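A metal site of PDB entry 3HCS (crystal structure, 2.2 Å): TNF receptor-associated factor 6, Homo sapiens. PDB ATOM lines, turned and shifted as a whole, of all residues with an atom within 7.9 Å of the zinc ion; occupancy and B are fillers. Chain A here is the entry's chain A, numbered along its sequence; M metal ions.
The side-chain sulfur of Cys 24 sits close to the backbone NH of Gly 6 (3.5 Å).
SG of Cys 24 lies close to N of Met 26.
SG of Cys 21 sits close to N of Ile 23, at 3.4 Å.
The backbone carbonyl oxygen (O) of Met 26 lies within hydrogen-bond range of the backbone NH (N) of Cys 21, at 2.8 Å.
SG of Cys 41 lies close to N of Arg 29 (3.3 Å).
Four residues have an atom within 4 Å of the zinc ion: Cys 21, Cys 24, Cys 41 and Cys 44.
The nearest printed residue that does not touch the zinc ion is Gly 6 (4.3 Å).
The zinc ion is bound by the side-chain sulfur (SG) of Cys 44 (2.5 Å), the side-chain sulfur (SG) of Cys 24 (2.5 Å), the side-chain sulfur (SG) of Cys 21 (2.5 Å) and the side-chain sulfur (SG) of Cys 41 (2.6 Å).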
ATOM      1  N   GLN A   5      -9.181   8.293  13.639  1.00  0.00           N
ATOM      2  CA  GLN A   5      -9.926   8.187  12.357  1.00  0.00           C
ATOM      3  C   GLN A   5      -8.963   8.386  11.178  1.00  0.00           C
ATOM      4  O   GLN A   5      -9.372   8.379  10.027  1.00  0.00           O
ATOM      5  CB  GLN A   5     -11.016   9.272  12.329  1.00  0.00           C
ATOM      6  CG  GLN A   5     -12.082   9.104  11.265  1.00  0.00           C
ATOM      7  CD  GLN A   5     -12.992   7.928  11.542  1.00  0.00           C
ATOM      8  OE1 GLN A   5     -12.548   6.775  11.525  1.00  0.00           O
ATOM      9  NE2 GLN A   5     -14.261   8.204  11.813  1.00  0.00           N
ATOM     10  N   GLY A   6      -7.677   8.563  11.487  1.00  0.00           N
ATOM     11  CA  GLY A   6      -6.690   8.765  10.436  1.00  0.00           C
ATOM     12  C   GLY A   6      -6.371   7.479   9.687  1.00  0.00           C
ATOM     13  O   GLY A   6      -6.891   6.414  10.028  1.00  0.00           O
ATOM     14  N   TYR A   7      -5.514   7.572   8.681  1.00  0.00           N
ATOM     15  CA  TYR A   7      -5.156   6.389   7.899  1.00  0.00           C
ATOM     16  C   TYR A   7      -4.429   5.335   8.728  1.00  0.00           C
ATOM     17  O   TYR A   7      -3.320   5.561   9.217  1.00  0.00           O
ATOM     18  CB  TYR A   7      -4.261   6.764   6.715  1.00  0.00           C
ATOM     19  CG  TYR A   7      -4.892   7.709   5.741  1.00  0.00           C
ATOM     20  CD1 TYR A   7      -4.579   9.066   5.757  1.00  0.00           C
ATOM     21  CD2 TYR A   7      -5.804   7.255   4.780  1.00  0.00           C
ATOM     22  CE1 TYR A   7      -5.148   9.939   4.851  1.00  0.00           C
ATOM     23  CE2 TYR A   7      -6.382   8.133   3.864  1.00  0.00           C
ATOM     24  CZ  TYR A   7      -6.042   9.473   3.909  1.00  0.00           C
ATOM     25  OH  TYR A   7      -6.588  10.357   3.019  1.00  0.00           O
ATOM     26  N   GLU A  20       1.545  12.783  11.738  1.00  0.00           N
ATOM     27  CA  GLU A  20       0.648  12.083  12.634  1.00  0.00           C
ATOM     28  C   GLU A  20      -0.326  13.041  13.320  1.00  0.00           C
ATOM     29  O   GLU A  20       0.030  14.159  13.673  1.00  0.00           O
ATOM     30  CB  GLU A  20       1.426  11.338  13.726  1.00  0.00           C
ATOM     31  CG  GLU A  20       2.080  10.053  13.268  1.00  0.00           C
ATOM     32  CD  GLU A  20       2.904   9.401  14.367  1.00  0.00           C
ATOM     33  OE1 GLU A  20       2.343   9.126  15.460  1.00  0.00           O
ATOM     34  OE2 GLU A  20       4.108   9.169  14.142  1.00  0.00           O
ATOM     35  N   CYS A  21      -1.560  12.592  13.481  1.00  0.00           N
ATOM     36  CA  CYS A  21      -2.565  13.395  14.152  1.00  0.00           C
ATOM     37  C   CYS A  21      -2.402  13.244  15.660  1.00  0.00           C
ATOM     38  O   CYS A  21      -2.415  12.135  16.183  1.00  0.00           O
ATOM     39  CB  CYS A  21      -3.955  12.939  13.747  1.00  0.00           C
ATOM     40  SG  CYS A  21      -5.217  13.813  14.668  1.00  0.00           S
ATOM     41  N   PRO A  22      -2.242  14.368  16.371  1.00  0.00           N
ATOM     42  CA  PRO A  22      -2.085  14.314  17.831  1.00  0.00           C
ATOM     43  C   PRO A  22      -3.230  13.617  18.546  1.00  0.00           C
ATOM     44  O   PRO A  22      -3.059  13.099  19.647  1.00  0.00           O
ATOM     45  CB  PRO A  22      -1.968  15.792  18.217  1.00  0.00           C
ATOM     46  CG  PRO A  22      -1.420  16.443  16.984  1.00  0.00           C
ATOM     47  CD  PRO A  22      -2.203  15.756  15.894  1.00  0.00           C
ATOM     48  N   ILE A  23      -4.407  13.595  17.929  1.00  0.00           N
ATOM     49  CA  ILE A  23      -5.567  12.970  18.559  1.00  0.00           C
ATOM     50  C   ILE A  23      -5.627  11.452  18.341  1.00  0.00           C
ATOM     51  O   ILE A  23      -5.519  10.680  19.298  1.00  0.00           O
ATOM     52  CB  ILE A  23      -6.881  13.601  18.070  1.00  0.00           C
ATOM     53  CG1 ILE A  23      -6.889  15.102  18.409  1.00  0.00           C
ATOM     54  CG2 ILE A  23      -8.063  12.911  18.739  1.00  0.00           C
ATOM     55  CD1 ILE A  23      -8.131  15.844  17.922  1.00  0.00           C
ATOM     56  N   CYS A  24      -5.797  11.024  17.092  1.00  0.00           N
ATOM     57  CA  CYS A  24      -5.900   9.588  16.793  1.00  0.00           C
ATOM     58  C   CYS A  24      -4.529   8.902  16.703  1.00  0.00           C
ATOM     59  O   CYS A  24      -4.446   7.679  16.767  1.00  0.00           O
ATOM     60  CB  CYS A  24      -6.644   9.387  15.477  1.00  0.00           C
ATOM     61  SG  CYS A  24      -5.649   9.848  14.061  1.00  0.00           S
ATOM     62  N   LEU A  25      -3.485   9.696  16.549  1.00  0.00           N
ATOM     63  CA  LEU A  25      -2.112   9.195  16.444  1.00  0.00           C
ATOM     64  C   LEU A  25      -1.804   8.405  15.173  1.00  0.00           C
ATOM     65  O   LEU A  25      -0.899   7.577  15.163  1.00  0.00           O
ATOM     66  CB  LEU A  25      -1.739   8.385  17.673  1.00  0.00           C
ATOM     67  CG  LEU A  25      -1.594   9.171  18.989  1.00  0.00           C
ATOM     68  CD1 LEU A  25      -0.993   8.262  20.045  1.00  0.00           C
ATOM     69  CD2 LEU A  25      -0.709  10.390  18.782  1.00  0.00           C
ATOM     70  N   MET A  26      -2.530   8.687  14.100  1.00  0.00           N
ATOM     71  CA  MET A  26      -2.307   8.035  12.819  1.00  0.00           C
ATOM     72  C   MET A  26      -2.128   9.113  11.741  1.00  0.00           C
ATOM     73  O   MET A  26      -2.304  10.299  12.015  1.00  0.00           O
ATOM     74  CB  MET A  26      -3.484   7.127  12.472  1.00  0.00           C
ATOM     75  CG  MET A  26      -3.697   6.041  13.504  1.00  0.00           C
ATOM     76  SD  MET A  26      -4.922   4.836  12.975  1.00  0.00           S
ATOM     77  CE  MET A  26      -6.466   5.735  13.333  1.00  0.00           C
ATOM     78  N   ALA A  27      -1.763   8.708  10.534  1.00  0.00           N
ATOM     79  CA  ALA A  27      -1.568   9.659   9.444  1.00  0.00           C
ATOM     80  C   ALA A  27      -2.807  10.527   9.260  1.00  0.00           C
ATOM     81  O   ALA A  27      -3.935  10.023   9.200  1.00  0.00           O
ATOM     82  CB  ALA A  27      -1.248   8.920   8.147  1.00  0.00           C
ATOM     83  N   LEU A  28      -2.601  11.834   9.183  1.00  0.00           N
ATOM     84  CA  LEU A  28      -3.680  12.797   9.002  1.00  0.00           C
ATOM     85  C   LEU A  28      -4.600  12.485   7.818  1.00  0.00           C
ATOM     86  O   LEU A  28      -4.128  12.279   6.693  1.00  0.00           O
ATOM     87  CB  LEU A  28      -3.105  14.202   8.830  1.00  0.00           C
ATOM     88  CG  LEU A  28      -2.185  14.702   9.938  1.00  0.00           C
ATOM     89  CD1 LEU A  28      -1.334  15.840   9.408  1.00  0.00           C
ATOM     90  CD2 LEU A  28      -3.017  15.140  11.141  1.00  0.00           C
ATOM     91  N   ARG A  29      -5.905  12.432   8.069  1.00  0.00           N
ATOM     92  CA  ARG A  29      -6.881  12.184   7.009  1.00  0.00           C
ATOM     93  C   ARG A  29      -7.641  13.482   6.862  1.00  0.00           C
ATOM     94  O   ARG A  29      -8.245  13.959   7.822  1.00  0.00           O
ATOM     95  CB  ARG A  29      -7.847  11.058   7.401  1.00  0.00           C
ATOM     96  CG  ARG A  29      -8.854  10.688   6.304  1.00  0.00           C
ATOM     97  CD  ARG A  29      -9.965   9.786   6.859  1.00  0.00           C
ATOM     98  NE  ARG A  29      -9.440   8.527   7.376  1.00  0.00           N
ATOM     99  CZ  ARG A  29      -9.132   7.475   6.630  1.00  0.00           C
ATOM    100  NH1 ARG A  29      -9.306   7.529   5.313  1.00  0.00           N
ATOM    101  NH2 ARG A  29      -8.625   6.386   7.186  1.00  0.00           N
ATOM    102  N   ARG A  39      -1.611  20.487  13.246  1.00  0.00           N
ATOM    103  CA  ARG A  39      -2.366  19.711  12.269  1.00  0.00           C
ATOM    104  C   ARG A  39      -3.171  18.593  12.893  1.00  0.00           C
ATOM    105  O   ARG A  39      -2.729  17.948  13.838  1.00  0.00           O
ATOM    106  CB  ARG A  39      -1.413  19.102  11.256  1.00  0.00           C
ATOM    107  CG  ARG A  39      -0.606  20.088  10.460  1.00  0.00           C
ATOM    108  CD  ARG A  39       0.572  19.338   9.894  1.00  0.00           C
ATOM    109  NE  ARG A  39       1.122  19.955   8.695  1.00  0.00           N
ATOM    110  CZ  ARG A  39       2.138  19.433   8.020  1.00  0.00           C
ATOM    111  NH1 ARG A  39       2.697  18.309   8.451  1.00  0.00           N
ATOM    112  NH2 ARG A  39       2.582  20.034   6.926  1.00  0.00           N
ATOM    113  N   PHE A  40      -4.358  18.352  12.345  1.00  0.00           N
ATOM    114  CA  PHE A  40      -5.242  17.292  12.823  1.00  0.00           C
ATOM    115  C   PHE A  40      -6.093  16.771  11.667  1.00  0.00           C
ATOM    116  O   PHE A  40      -6.204  17.414  10.610  1.00  0.00           O
ATOM    117  CB  PHE A  40      -6.211  17.809  13.886  1.00  0.00           C
ATOM    118  CG  PHE A  40      -5.561  18.461  15.077  1.00  0.00           C
ATOM    119  CD1 PHE A  40      -5.337  19.833  15.093  1.00  0.00           C
ATOM    120  CD2 PHE A  40      -5.244  17.701  16.208  1.00  0.00           C
ATOM    121  CE1 PHE A  40      -4.805  20.450  16.221  1.00  0.00           C
ATOM    122  CE2 PHE A  40      -4.711  18.319  17.346  1.00  0.00           C
ATOM    123  CZ  PHE A  40      -4.488  19.690  17.352  1.00  0.00           C
ATOM    124  N   CYS A  41      -6.683  15.593  11.854  1.00  0.00           N
ATOM    125  CA  CYS A  41      -7.576  15.053  10.846  1.00  0.00           C
ATOM    126  C   CYS A  41      -8.772  15.978  11.037  1.00  0.00           C
ATOM    127  O   CYS A  41      -9.071  16.360  12.177  1.00  0.00           O
ATOM    128  CB  CYS A  41      -7.989  13.616  11.173  1.00  0.00           C
ATOM    129  SG  CYS A  41      -6.646  12.398  11.239  1.00  0.00           S
ATOM    130  N   LYS A  42      -9.459  16.344   9.963  1.00  0.00           N
ATOM    131  CA  LYS A  42     -10.612  17.215  10.102  1.00  0.00           C
ATOM    132  C   LYS A  42     -11.630  16.661  11.103  1.00  0.00           C
ATOM    133  O   LYS A  42     -12.179  17.389  11.925  1.00  0.00           O
ATOM    134  CB  LYS A  42     -11.288  17.423   8.746  1.00  0.00           C
ATOM    135  CG  LYS A  42     -12.521  18.292   8.814  1.00  0.00           C
ATOM    136  CD  LYS A  42     -12.992  18.722   7.445  1.00  0.00           C
ATOM    137  CE  LYS A  42     -14.091  19.765   7.564  1.00  0.00           C
ATOM    138  NZ  LYS A  42     -14.377  20.448   6.273  1.00  0.00           N
ATOM    139  N   ALA A  43     -11.848  15.352  11.041  1.00  0.00           N
ATOM    140  CA  ALA A  43     -12.810  14.684  11.912  1.00  0.00           C
ATOM    141  C   ALA A  43     -12.425  14.663  13.382  1.00  0.00           C
ATOM    142  O   ALA A  43     -13.268  14.815  14.265  1.00  0.00           O
ATOM    143  CB  ALA A  43     -13.071  13.257  11.420  1.00  0.00           C
ATOM    144  N   CYS A  44     -11.146  14.421  13.643  1.00  0.00           N
ATOM    145  CA  CYS A  44     -10.682  14.363  15.024  1.00  0.00           C
ATOM    146  C   CYS A  44     -10.731  15.709  15.745  1.00  0.00           C
ATOM    147  O   CYS A  44     -11.172  15.770  16.898  1.00  0.00           O
ATOM    148  CB  CYS A  44      -9.263  13.793  15.081  1.00  0.00           C
ATOM    149  SG  CYS A  44      -9.160  12.076  14.484  1.00  0.00           S
ATOM    150  N   ILE A  45     -10.283  16.773  15.089  1.00  0.00           N
ATOM    151  CA  ILE A  45     -10.300  18.088  15.707  1.00  0.00           C
ATOM    152  C   ILE A  45     -11.719  18.602  15.907  1.00  0.00           C
ATOM    153  O   ILE A  45     -12.029  19.212  16.930  1.00  0.00           O
ATOM    154  CB  ILE A  45      -9.474  19.119  14.885  1.00  0.00           C
ATOM    155  CG1 ILE A  45      -9.428  20.457  15.614  1.00  0.00           C
ATOM    156  CG2 ILE A  45     -10.054  19.273  13.490  1.00  0.00           C
ATOM    157  CD1 ILE A  45      -8.698  20.406  16.940  1.00  0.00           C
HETATM  158 ZN    ZN M   1      -6.771  12.054  13.809  1.00  0.00          ZN
